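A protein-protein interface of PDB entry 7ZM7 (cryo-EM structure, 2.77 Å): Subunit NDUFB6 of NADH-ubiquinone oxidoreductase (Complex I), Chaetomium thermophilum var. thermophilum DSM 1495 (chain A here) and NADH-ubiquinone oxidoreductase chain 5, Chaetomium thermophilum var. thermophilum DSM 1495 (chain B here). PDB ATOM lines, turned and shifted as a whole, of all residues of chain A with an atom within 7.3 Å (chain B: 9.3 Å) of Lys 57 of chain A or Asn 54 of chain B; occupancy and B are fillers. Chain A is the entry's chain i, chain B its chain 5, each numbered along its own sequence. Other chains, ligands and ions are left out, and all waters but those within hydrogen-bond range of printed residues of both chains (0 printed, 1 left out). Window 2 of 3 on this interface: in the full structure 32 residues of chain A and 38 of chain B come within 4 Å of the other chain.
The backbone NH of Val 54 of chain A sits at hydrogen-bond distance from the backbone carbonyl oxygen of Thr 58 of chain B (2.8 Å).
NZ of Lys 57 of chain A sits at hydrogen-bond distance from O of Asn 53 of chain B, 3.0 Å away.
The guanidinium group of Arg 63 of chain A is in hydrogen-bond range of the backbone carbonyl oxygen of Phe 52 of chain B, 2.6 Å away.
The side-chain hydroxyl of Tyr 65 of chain A sits close to the side-chain carboxylate of Glu 49 of chain B (3.4 Å).
Hydrophobic or aromatic side chains of chain B that line the printed part of chain A: Ile 55 and Val 57.
OH of Tyr 65 of chain A lies within hydrogen-bond range of NH2 of Arg 55 of chain A (2.9 Å).
The side-chain amide nitrogen (NE2) of Gln 73 of chain A is in hydrogen-bond range of the backbone carbonyl oxygen (O) of Arg 55 of chain A (2.9 Å).
O of Phe 48 of chain B lies within hydrogen-bond range of ND2 of Asn 53 of chain B, 3.1 Å away.
The side-chain amide nitrogen of Asn 53 of chain B sits at hydrogen-bond distance from the backbone carbonyl oxygen of Glu 49 of chain B (3.3 Å).
O of Val 50 of chain B sits at hydrogen-bond distance from N of Ile 55 of chain B (3.1 Å).
N of Tyr 78 of chain B sits at hydrogen-bond distance from O of Val 57 of chain B (2.7 Å).
Lys 57 of chain A touches just these residues of chain B: Asn 53 (3.0 Å), Asn 54 (3.5 Å) and Ile 55 (3.4 Å).
No residue of chain B comes within 4 Å of Met 58 of chain A.
Of the printed residues of chain A, Val 57 of chain B touches Val 54 and Arg 55.
Printed residues of chain A within 4 Å of Thr 58 of chain B: Val 54.
Asn 498 of chain B touches none of the printed residues of chain A.
The nearest residue of chain B that does not touch Lys 57 of chain A is Pro 56 of chain B (5.5 Å).
Among the printed residues, merely in contact across the chains: Arg 55 of chain A with Val 57 of chain B, Arg 63 of chain A with Asn 53 of chain B, Lys 57 of chain A with Ile 55 of chain B, Lys 57 of chain A with Asn 54 of chain B, Tyr 65 of chain A with Asn 53 of chain B, Tyr 65 of chain A with Ile 55 of chain B, Pro 59 of chain A with Ile 55 of chain B, Arg 55 of chain A with Ile 55 of chain B, Val 54 of chain A with Val 57 of chain B and Val 54 of chain A with Pro 56 of chain B.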
ATOM      1  N   VAL A  54      -8.840   9.075  -3.073  1.00  0.00           N
ATOM      2  CA  VAL A  54      -8.049   8.067  -2.382  1.00  0.00           C
ATOM      3  C   VAL A  54      -8.831   7.548  -1.185  1.00  0.00           C
ATOM      4  O   VAL A  54      -9.138   8.304  -0.259  1.00  0.00           O
ATOM      5  CB  VAL A  54      -6.688   8.622  -1.954  1.00  0.00           C
ATOM      6  CG1 VAL A  54      -6.037   7.701  -0.954  1.00  0.00           C
ATOM      7  CG2 VAL A  54      -5.808   8.782  -3.168  1.00  0.00           C
ATOM      8  N   ARG A  55      -9.132   6.252  -1.198  1.00  0.00           N
ATOM      9  CA  ARG A  55      -9.835   5.584  -0.114  1.00  0.00           C
ATOM     10  C   ARG A  55      -8.977   4.448   0.400  1.00  0.00           C
ATOM     11  O   ARG A  55      -8.395   3.702  -0.389  1.00  0.00           O
ATOM     12  CB  ARG A  55     -11.188   5.044  -0.573  1.00  0.00           C
ATOM     13  CG  ARG A  55     -12.047   6.026  -1.342  1.00  0.00           C
ATOM     14  CD  ARG A  55     -13.285   5.340  -1.880  1.00  0.00           C
ATOM     15  NE  ARG A  55     -13.716   5.889  -3.163  1.00  0.00           N
ATOM     16  CZ  ARG A  55     -14.472   6.969  -3.300  1.00  0.00           C
ATOM     17  NH1 ARG A  55     -14.823   7.395  -4.497  1.00  0.00           N
ATOM     18  NH2 ARG A  55     -14.908   7.614  -2.242  1.00  0.00           N
ATOM     19  N   HIS A  56      -8.965   4.273   1.719  1.00  0.00           N
ATOM     20  CA  HIS A  56      -8.167   3.193   2.349  1.00  0.00           C
ATOM     21  C   HIS A  56      -9.106   2.044   2.697  1.00  0.00           C
ATOM     22  O   HIS A  56      -8.599   0.969   3.063  1.00  0.00           O
ATOM     23  CB  HIS A  56      -7.434   3.742   3.574  1.00  0.00           C
ATOM     24  CG  HIS A  56      -6.625   4.963   3.302  1.00  0.00           C
ATOM     25  ND1 HIS A  56      -5.324   4.897   2.858  1.00  0.00           N
ATOM     26  CD2 HIS A  56      -6.923   6.274   3.416  1.00  0.00           C
ATOM     27  CE1 HIS A  56      -4.855   6.118   2.704  1.00  0.00           C
ATOM     28  NE2 HIS A  56      -5.815   6.980   3.041  1.00  0.00           N
ATOM     29  N   LYS A  57     -10.415   2.260   2.585  1.00  0.00           N
ATOM     30  CA  LYS A  57     -11.376   1.210   2.858  1.00  0.00           C
ATOM     31  C   LYS A  57     -12.172   0.938   1.597  1.00  0.00           C
ATOM     32  O   LYS A  57     -12.408   1.835   0.789  1.00  0.00           O
ATOM     33  CB  LYS A  57     -12.314   1.574   4.008  1.00  0.00           C
ATOM     34  CG  LYS A  57     -13.016   0.380   4.632  1.00  0.00           C
ATOM     35  CD  LYS A  57     -13.228   0.584   6.119  1.00  0.00           C
ATOM     36  CE  LYS A  57     -14.333  -0.311   6.652  1.00  0.00           C
ATOM     37  NZ  LYS A  57     -15.655   0.044   6.062  1.00  0.00           N
ATOM     38  N   MET A  58     -12.550  -0.299   1.422  1.00  0.00           N
ATOM     39  CA  MET A  58     -13.215  -0.545   0.166  1.00  0.00           C
ATOM     40  C   MET A  58     -14.676  -0.881   0.390  1.00  0.00           C
ATOM     41  O   MET A  58     -15.016  -1.555   1.368  1.00  0.00           O
ATOM     42  CB  MET A  58     -12.542  -1.687  -0.588  1.00  0.00           C
ATOM     43  CG  MET A  58     -11.143  -1.336  -1.000  1.00  0.00           C
ATOM     44  SD  MET A  58     -11.258   0.093  -2.067  1.00  0.00           S
ATOM     45  CE  MET A  58     -12.041  -0.681  -3.447  1.00  0.00           C
ATOM     46  N   PRO A  59     -15.554  -0.426  -0.490  1.00  0.00           N
ATOM     47  CA  PRO A  59     -16.986  -0.631  -0.273  1.00  0.00           C
ATOM     48  C   PRO A  59     -17.358  -2.096  -0.356  1.00  0.00           C
ATOM     49  O   PRO A  59     -16.715  -2.887  -1.048  1.00  0.00           O
ATOM     50  CB  PRO A  59     -17.634   0.169  -1.408  1.00  0.00           C
ATOM     51  CG  PRO A  59     -16.558   1.076  -1.909  1.00  0.00           C
ATOM     52  CD  PRO A  59     -15.285   0.344  -1.707  1.00  0.00           C
ATOM     53  N   GLU A  60     -18.413  -2.453   0.362  1.00  0.00           N
ATOM     54  CA  GLU A  60     -18.916  -3.813   0.321  1.00  0.00           C
ATOM     55  C   GLU A  60     -19.504  -4.122  -1.055  1.00  0.00           C
ATOM     56  O   GLU A  60     -19.958  -3.219  -1.763  1.00  0.00           O
ATOM     57  CB  GLU A  60     -19.972  -4.016   1.401  1.00  0.00           C
ATOM     58  CG  GLU A  60     -19.418  -3.982   2.808  1.00  0.00           C
ATOM     59  CD  GLU A  60     -18.677  -5.249   3.162  1.00  0.00           C
ATOM     60  OE1 GLU A  60     -18.997  -6.303   2.576  1.00  0.00           O
ATOM     61  OE2 GLU A  60     -17.783  -5.195   4.029  1.00  0.00           O
ATOM     62  N   ARG A  63     -23.738  -3.177  -1.022  1.00  0.00           N
ATOM     63  CA  ARG A  63     -24.409  -1.974  -0.555  1.00  0.00           C
ATOM     64  C   ARG A  63     -24.257  -0.818  -1.539  1.00  0.00           C
ATOM     65  O   ARG A  63     -23.268  -0.717  -2.267  1.00  0.00           O
ATOM     66  CB  ARG A  63     -23.906  -1.552   0.825  1.00  0.00           C
ATOM     67  CG  ARG A  63     -24.666  -0.341   1.302  1.00  0.00           C
ATOM     68  CD  ARG A  63     -24.354   0.156   2.671  1.00  0.00           C
ATOM     69  NE  ARG A  63     -24.789  -0.777   3.696  1.00  0.00           N
ATOM     70  CZ  ARG A  63     -24.489  -0.639   4.978  1.00  0.00           C
ATOM     71  NH1 ARG A  63     -24.917  -1.522   5.869  1.00  0.00           N
ATOM     72  NH2 ARG A  63     -23.809   0.427   5.372  1.00  0.00           N
ATOM     73  N   TYR A  65     -23.437   2.309  -3.418  1.00  0.00           N
ATOM     74  CA  TYR A  65     -22.223   3.117  -3.436  1.00  0.00           C
ATOM     75  C   TYR A  65     -21.963   3.495  -4.884  1.00  0.00           C
ATOM     76  O   TYR A  65     -21.099   2.917  -5.552  1.00  0.00           O
ATOM     77  CB  TYR A  65     -21.053   2.346  -2.835  1.00  0.00           C
ATOM     78  CG  TYR A  65     -19.858   3.164  -2.430  1.00  0.00           C
ATOM     79  CD1 TYR A  65     -18.821   3.399  -3.316  1.00  0.00           C
ATOM     80  CD2 TYR A  65     -19.753   3.682  -1.158  1.00  0.00           C
ATOM     81  CE1 TYR A  65     -17.716   4.135  -2.946  1.00  0.00           C
ATOM     82  CE2 TYR A  65     -18.659   4.413  -0.778  1.00  0.00           C
ATOM     83  CZ  TYR A  65     -17.642   4.640  -1.680  1.00  0.00           C
ATOM     84  OH  TYR A  65     -16.552   5.376  -1.306  1.00  0.00           O
ATOM     85  N   GLN A  73      -9.769   3.674  -8.474  1.00  0.00           N
ATOM     86  CA  GLN A  73      -9.157   2.849  -7.407  1.00  0.00           C
ATOM     87  C   GLN A  73     -10.143   1.754  -7.026  1.00  0.00           C
ATOM     88  O   GLN A  73      -9.717   0.601  -6.897  1.00  0.00           O
ATOM     89  CB  GLN A  73      -8.827   3.724  -6.199  1.00  0.00           C
ATOM     90  CG  GLN A  73      -8.094   2.992  -5.086  1.00  0.00           C
ATOM     91  CD  GLN A  73      -7.975   3.845  -3.849  1.00  0.00           C
ATOM     92  OE1 GLN A  73      -8.668   4.849  -3.695  1.00  0.00           O
ATOM     93  NE2 GLN A  73      -7.092   3.445  -2.950  1.00  0.00           N
ATOM     94  N   ILE A  74     -11.418   2.112  -6.904  1.00  0.00           N
ATOM     95  CA  ILE A  74     -12.443   1.118  -6.481  1.00  0.00           C
ATOM     96  C   ILE A  74     -12.691   0.180  -7.637  1.00  0.00           C
ATOM     97  O   ILE A  74     -12.749  -1.024  -7.422  1.00  0.00           O
ATOM     98  CB  ILE A  74     -13.754   1.809  -6.074  1.00  0.00           C
ATOM     99  CG1 ILE A  74     -13.599   2.575  -4.763  1.00  0.00           C
ATOM    100  CG2 ILE A  74     -14.889   0.805  -5.991  1.00  0.00           C
ATOM    101  CD1 ILE A  74     -14.902   3.104  -4.257  1.00  0.00           C
ATOM    102  N   ALA B  46     -23.175  11.689  -1.015  1.00  0.00           N
ATOM    103  CA  ALA B  46     -21.922  11.557  -0.282  1.00  0.00           C
ATOM    104  C   ALA B  46     -22.148  11.207   1.179  1.00  0.00           C
ATOM    105  O   ALA B  46     -21.253  10.661   1.826  1.00  0.00           O
ATOM    106  CB  ALA B  46     -21.113  12.841  -0.392  1.00  0.00           C
ATOM    107  N   PHE B  47     -23.312  11.533   1.732  1.00  0.00           N
ATOM    108  CA  PHE B  47     -23.556  11.175   3.121  1.00  0.00           C
ATOM    109  C   PHE B  47     -23.692   9.667   3.267  1.00  0.00           C
ATOM    110  O   PHE B  47     -23.130   9.072   4.190  1.00  0.00           O
ATOM    111  CB  PHE B  47     -24.792  11.895   3.643  1.00  0.00           C
ATOM    112  CG  PHE B  47     -24.922  11.862   5.133  1.00  0.00           C
ATOM    113  CD1 PHE B  47     -25.585  10.827   5.760  1.00  0.00           C
ATOM    114  CD2 PHE B  47     -24.370  12.864   5.913  1.00  0.00           C
ATOM    115  CE1 PHE B  47     -25.698  10.794   7.123  1.00  0.00           C
ATOM    116  CE2 PHE B  47     -24.482  12.836   7.284  1.00  0.00           C
ATOM    117  CZ  PHE B  47     -25.150  11.802   7.887  1.00  0.00           C
ATOM    118  N   PHE B  48     -24.494   9.058   2.405  1.00  0.00           N
ATOM    119  CA  PHE B  48     -24.636   7.586   2.451  1.00  0.00           C
ATOM    120  C   PHE B  48     -23.277   6.978   2.123  1.00  0.00           C
ATOM    121  O   PHE B  48     -22.844   6.046   2.806  1.00  0.00           O
ATOM    122  CB  PHE B  48     -25.737   7.137   1.492  1.00  0.00           C
ATOM    123  CG  PHE B  48     -27.137   7.456   1.951  1.00  0.00           C
ATOM    124  CD1 PHE B  48     -27.927   6.482   2.539  1.00  0.00           C
ATOM    125  CD2 PHE B  48     -27.665   8.726   1.798  1.00  0.00           C
ATOM    126  CE1 PHE B  48     -29.214   6.773   2.963  1.00  0.00           C
ATOM    127  CE2 PHE B  48     -28.951   9.017   2.222  1.00  0.00           C
ATOM    128  CZ  PHE B  48     -29.723   8.040   2.803  1.00  0.00           C
ATOM    129  N   GLU B  49     -22.609   7.529   1.122  1.00  0.00           N
ATOM    130  CA  GLU B  49     -21.312   6.980   0.669  1.00  0.00           C
ATOM    131  C   GLU B  49     -20.225   7.028   1.739  1.00  0.00           C
ATOM    132  O   GLU B  49     -19.570   6.002   1.927  1.00  0.00           O
ATOM    133  CB  GLU B  49     -20.831   7.889  -0.455  1.00  0.00           C
ATOM    134  CG  GLU B  49     -21.435   7.555  -1.792  1.00  0.00           C
ATOM    135  CD  GLU B  49     -20.366   6.966  -2.680  1.00  0.00           C
ATOM    136  OE1 GLU B  49     -19.191   7.275  -2.446  1.00  0.00           O
ATOM    137  OE2 GLU B  49     -20.703   6.186  -3.569  1.00  0.00           O
ATOM    138  N   VAL B  50     -20.049   8.147   2.438  1.00  0.00           N
ATOM    139  CA  VAL B  50     -18.883   8.258   3.366  1.00  0.00           C
ATOM    140  C   VAL B  50     -19.270   7.783   4.753  1.00  0.00           C
ATOM    141  O   VAL B  50     -18.543   6.935   5.299  1.00  0.00           O
ATOM    142  CB  VAL B  50     -18.315   9.688   3.410  1.00  0.00           C
ATOM    143  CG1 VAL B  50     -17.229   9.845   4.460  1.00  0.00           C
ATOM    144  CG2 VAL B  50     -17.805  10.135   2.051  1.00  0.00           C
ATOM    145  N   GLY B  51     -20.382   8.284   5.277  1.00  0.00           N
ATOM    146  CA  GLY B  51     -20.769   7.977   6.642  1.00  0.00           C
ATOM    147  C   GLY B  51     -21.296   6.570   6.808  1.00  0.00           C
ATOM    148  O   GLY B  51     -20.896   5.850   7.724  1.00  0.00           O
ATOM    149  N   PHE B  52     -22.199   6.156   5.929  1.00  0.00           N
ATOM    150  CA  PHE B  52     -22.873   4.885   6.139  1.00  0.00           C
ATOM    151  C   PHE B  52     -22.019   3.707   5.711  1.00  0.00           C
ATOM    152  O   PHE B  52     -22.467   2.561   5.789  1.00  0.00           O
ATOM    153  CB  PHE B  52     -24.212   4.874   5.416  1.00  0.00           C
ATOM    154  CG  PHE B  52     -25.274   5.631   6.134  1.00  0.00           C
ATOM    155  CD1 PHE B  52     -25.762   5.171   7.341  1.00  0.00           C
ATOM    156  CD2 PHE B  52     -25.780   6.801   5.617  1.00  0.00           C
ATOM    157  CE1 PHE B  52     -26.739   5.863   8.015  1.00  0.00           C
ATOM    158  CE2 PHE B  52     -26.755   7.494   6.287  1.00  0.00           C
ATOM    159  CZ  PHE B  52     -27.236   7.025   7.487  1.00  0.00           C
ATOM    160  N   ASN B  53     -20.808   3.959   5.243  1.00  0.00           N
ATOM    161  CA  ASN B  53     -19.881   2.895   4.904  1.00  0.00           C
ATOM    162  C   ASN B  53     -18.532   3.049   5.584  1.00  0.00           C
ATOM    163  O   ASN B  53     -17.677   2.172   5.431  1.00  0.00           O
ATOM    164  CB  ASN B  53     -19.704   2.828   3.397  1.00  0.00           C
ATOM    165  CG  ASN B  53     -20.964   2.419   2.698  1.00  0.00           C
ATOM    166  OD1 ASN B  53     -21.415   1.289   2.838  1.00  0.00           O
ATOM    167  ND2 ASN B  53     -21.560   3.345   1.954  1.00  0.00           N
ATOM    168  N   ASN B  54     -18.331   4.131   6.335  1.00  0.00           N
ATOM    169  CA  ASN B  54     -17.087   4.384   7.048  1.00  0.00           C
ATOM    170  C   ASN B  54     -15.919   4.355   6.070  1.00  0.00           C
ATOM    171  O   ASN B  54     -14.921   3.659   6.256  1.00  0.00           O
ATOM    172  CB  ASN B  54     -16.900   3.384   8.191  1.00  0.00           C
ATOM    173  CG  ASN B  54     -15.596   3.576   8.938  1.00  0.00           C
ATOM    174  OD1 ASN B  54     -15.132   4.701   9.119  1.00  0.00           O
ATOM    175  ND2 ASN B  54     -14.995   2.475   9.372  1.00  0.00           N
ATOM    176  N   ILE B  55     -16.074   5.109   4.988  1.00  0.00           N
ATOM    177  CA  ILE B  55     -15.045   5.210   3.961  1.00  0.00           C
ATOM    178  C   ILE B  55     -14.673   6.669   3.774  1.00  0.00           C
ATOM    179  O   ILE B  55     -15.254   7.346   2.924  1.00  0.00           O
ATOM    180  CB  ILE B  55     -15.507   4.600   2.634  1.00  0.00           C
ATOM    181  CG1 ILE B  55     -16.085   3.212   2.856  1.00  0.00           C
ATOM    182  CG2 ILE B  55     -14.369   4.516   1.661  1.00  0.00           C
ATOM    183  CD1 ILE B  55     -16.593   2.574   1.580  1.00  0.00           C
ATOM    184  N   PRO B  56     -13.737   7.196   4.551  1.00  0.00           N
ATOM    185  CA  PRO B  56     -13.275   8.562   4.314  1.00  0.00           C
ATOM    186  C   PRO B  56     -12.665   8.702   2.931  1.00  0.00           C
ATOM    187  O   PRO B  56     -12.081   7.763   2.390  1.00  0.00           O
ATOM    188  CB  PRO B  56     -12.239   8.770   5.415  1.00  0.00           C
ATOM    189  CG  PRO B  56     -12.677   7.871   6.480  1.00  0.00           C
ATOM    190  CD  PRO B  56     -13.181   6.652   5.795  1.00  0.00           C
ATOM    191  N   VAL B  57     -12.824   9.882   2.348  1.00  0.00           N
ATOM    192  CA  VAL B  57     -12.345  10.164   1.004  1.00  0.00           C
ATOM    193  C   VAL B  57     -11.275  11.243   1.098  1.00  0.00           C
ATOM    194  O   VAL B  57     -11.475  12.273   1.751  1.00  0.00           O
ATOM    195  CB  VAL B  57     -13.492  10.618   0.089  1.00  0.00           C
ATOM    196  CG1 VAL B  57     -12.975  10.964  -1.281  1.00  0.00           C
ATOM    197  CG2 VAL B  57     -14.577   9.595   0.061  1.00  0.00           C
ATOM    198  N   THR B  58     -10.142  11.008   0.460  1.00  0.00           N
ATOM    199  CA  THR B  58      -9.071  11.990   0.385  1.00  0.00           C
ATOM    200  C   THR B  58      -8.895  12.420  -1.060  1.00  0.00           C
ATOM    201  O   THR B  58      -9.029  11.601  -1.970  1.00  0.00           O
ATOM    202  CB  THR B  58      -7.761  11.420   0.925  1.00  0.00           C
ATOM    203  OG1 THR B  58      -7.986  10.806   2.199  1.00  0.00           O
ATOM    204  CG2 THR B  58      -6.737  12.502   1.074  1.00  0.00           C
ATOM    205  N   TYR B  78     -13.039  14.047   3.045  1.00  0.00           N
ATOM    206  CA  TYR B  78     -14.439  13.828   3.379  1.00  0.00           C
ATOM    207  C   TYR B  78     -14.520  12.733   4.427  1.00  0.00           C
ATOM    208  O   TYR B  78     -14.145  11.588   4.167  1.00  0.00           O
ATOM    209  CB  TYR B  78     -15.247  13.446   2.150  1.00  0.00           C
ATOM    210  CG  TYR B  78     -15.544  14.584   1.232  1.00  0.00           C
ATOM    211  CD1 TYR B  78     -14.611  15.002   0.302  1.00  0.00           C
ATOM    212  CD2 TYR B  78     -16.757  15.241   1.282  1.00  0.00           C
ATOM    213  CE1 TYR B  78     -14.872  16.034  -0.548  1.00  0.00           C
ATOM    214  CE2 TYR B  78     -17.025  16.280   0.429  1.00  0.00           C
ATOM    215  CZ  TYR B  78     -16.076  16.667  -0.486  1.00  0.00           C
ATOM    216  OH  TYR B  78     -16.329  17.703  -1.332  1.00  0.00           O
ATOM    217  N   ASP B  79     -15.017  13.084   5.605  1.00  0.00           N
ATOM    218  CA  ASP B  79     -15.145  12.137   6.696  1.00  0.00           C
ATOM    219  C   ASP B  79     -16.532  12.233   7.309  1.00  0.00           C
ATOM    220  O   ASP B  79     -17.406  12.913   6.773  1.00  0.00           O
ATOM    221  CB  ASP B  79     -14.058  12.375   7.742  1.00  0.00           C
ATOM    222  CG  ASP B  79     -14.041  13.805   8.263  1.00  0.00           C
ATOM    223  OD1 ASP B  79     -15.034  14.275   8.850  1.00  0.00           O
ATOM    224  OD2 ASP B  79     -13.007  14.471   8.082  1.00  0.00           O
ATOM    225  N   SER B  80     -16.731  11.557   8.435  1.00  0.00           N
ATOM    226  CA  SER B  80     -18.047  11.496   9.050  1.00  0.00           C
ATOM    227  C   SER B  80     -18.535  12.877   9.464  1.00  0.00           C
ATOM    228  O   SER B  80     -19.707  13.210   9.271  1.00  0.00           O
ATOM    229  CB  SER B  80     -17.998  10.554  10.250  1.00  0.00           C
ATOM    230  OG  SER B  80     -19.288  10.133  10.635  1.00  0.00           O
ATOM    231  N   VAL B  83     -19.540  15.302   6.173  1.00  0.00           N
ATOM    232  CA  VAL B  83     -20.798  15.070   5.487  1.00  0.00           C
ATOM    233  C   VAL B  83     -21.974  15.459   6.361  1.00  0.00           C
ATOM    234  O   VAL B  83     -23.032  15.837   5.851  1.00  0.00           O
ATOM    235  CB  VAL B  83     -20.859  13.607   5.047  1.00  0.00           C
ATOM    236  CG1 VAL B  83     -19.738  13.344   4.102  1.00  0.00           C
ATOM    237  CG2 VAL B  83     -20.755  12.699   6.252  1.00  0.00           C
ATOM    238  N   ASN B 498     -21.256   4.075  16.320  1.00  0.00           N
ATOM    239  CA  ASN B 498     -19.935   4.172  15.724  1.00  0.00           C
ATOM    240  C   ASN B 498     -19.970   4.929  14.401  1.00  0.00           C
ATOM    241  O   ASN B 498     -19.322   4.538  13.434  1.00  0.00           O
ATOM    242  CB  ASN B 498     -19.347   2.782  15.530  1.00  0.00           C
ATOM    243  CG  ASN B 498     -20.263   1.879  14.746  1.00  0.00           C
ATOM    244  OD1 ASN B 498     -21.469   2.105  14.693  1.00  0.00           O
ATOM    245  ND2 ASN B 498     -19.700   0.846  14.135  1.00  0.00           N
ATOM    246  N   PHE B 499     -20.695   6.044  14.346  1.00  0.00           N
ATOM    247  CA  PHE B 499     -20.686   6.843  13.097  1.00  0.00           C
ATOM    248  C   PHE B 499     -19.356   7.586  13.010  1.00  0.00           C
ATOM    249  O   PHE B 499     -18.683   7.503  11.962  1.00  0.00           O
ATOM    250  CB  PHE B 499     -21.860   7.817  13.019  1.00  0.00           C
ATOM    251  CG  PHE B 499     -22.259   8.259  11.634  1.00  0.00           C
ATOM    252  CD1 PHE B 499     -22.721   7.344  10.703  1.00  0.00           C
ATOM    253  CD2 PHE B 499     -22.212   9.593  11.273  1.00  0.00           C
ATOM    254  CE1 PHE B 499     -23.109   7.753   9.438  1.00  0.00           C
ATOM    255  CE2 PHE B 499     -22.590  10.002  10.004  1.00  0.00           C
ATOM    256  CZ  PHE B 499     -23.039   9.080   9.090  1.00  0.00           C
ATOM    257  N   PHE B 500     -18.993   8.292  14.075  1.00  0.00           N
ATOM    258  CA  PHE B 500     -17.722   9.051  14.087  1.00  0.00           C
ATOM    259  C   PHE B 500     -16.598   8.163  14.642  1.00  0.00           C
ATOM    260  O   PHE B 500     -16.061   8.505  15.705  1.00  0.00           O
ATOM    261  CB  PHE B 500     -17.968  10.377  14.818  1.00  0.00           C
ATOM    262  CG  PHE B 500     -19.328  10.965  14.538  1.00  0.00           C
ATOM    263  CD1 PHE B 500     -19.567  11.677  13.374  1.00  0.00           C
ATOM    264  CD2 PHE B 500     -20.379  10.782  15.423  1.00  0.00           C
ATOM    265  CE1 PHE B 500     -20.822  12.196  13.104  1.00  0.00           C
ATOM    266  CE2 PHE B 500     -21.633  11.306  15.154  1.00  0.00           C
ATOM    267  CZ  PHE B 500     -21.853  12.009  13.994  1.00  0.00           C
ATOM    268  N   VAL B 501     -16.239   7.082  13.941  1.00  0.00           N
ATOM    269  CA  VAL B 501     -15.189   6.123  14.417  1.00  0.00           C
ATOM    270  C   VAL B 501     -13.905   6.317  13.610  1.00  0.00           C
ATOM    271  O   VAL B 501     -12.995   5.482  13.717  1.00  0.00           O
ATOM    272  CB  VAL B 501     -15.709   4.678  14.374  1.00  0.00           C
ATOM    273  CG1 VAL B 501     -15.676   4.072  12.978  1.00  0.00           C
ATOM    274  CG2 VAL B 501     -15.022   3.787  15.389  1.00  0.00           C
ATOM    275  N   ASP B 502     -13.846   7.380  12.811  1.00  0.00           N
ATOM    276  CA  ASP B 502     -12.620   7.708  12.037  1.00  0.00           C
ATOM    277  C   ASP B 502     -11.870   8.781  12.826  1.00  0.00           C
ATOM    278  O   ASP B 502     -11.067   9.491  12.207  1.00  0.00           O
ATOM    279  CB  ASP B 502     -12.957   8.098  10.596  1.00  0.00           C
ATOM    280  CG  ASP B 502     -14.153   9.025  10.446  1.00  0.00           C
ATOM    281  OD1 ASP B 502     -14.657   9.519  11.474  1.00  0.00           O
ATOM    282  OD2 ASP B 502     -14.577   9.245   9.295  1.00  0.00           O
ATOM    283  N   ASN B 503     -12.224   8.958  14.105  1.00  0.00           N
ATOM    284  CA  ASN B 503     -11.570   9.951  14.998  1.00  0.00           C
ATOM    285  C   ASN B 503     -12.022  11.359  14.595  1.00  0.00           C
ATOM    286  O   ASN B 503     -11.346  12.320  14.990  1.00  0.00           O
ATOM    287  CB  ASN B 503     -10.049   9.772  15.091  1.00  0.00           C
ATOM    288  CG  ASN B 503      -9.493   9.924  16.489  1.00  0.00           C
ATOM    289  OD1 ASN B 503      -8.617  10.751  16.724  1.00  0.00           O
ATOM    290  ND2 ASN B 503      -9.990   9.125  17.418  1.00  0.00           N
ATOM    291  N   SER B 504     -13.107  11.477  13.830  1.00  0.00           N
ATOM    292  CA  SER B 504     -13.634  12.827  13.500  1.00  0.00           C
ATOM    293  C   SER B 504     -14.105  13.487  14.792  1.00  0.00           C
ATOM    294  O   SER B 504     -13.861  14.698  14.949  1.00  0.00           O
ATOM    295  CB  SER B 504     -14.711  12.814  12.442  1.00  0.00           C
ATOM    296  OG  SER B 504     -14.224  12.281  11.223  1.00  0.00           O
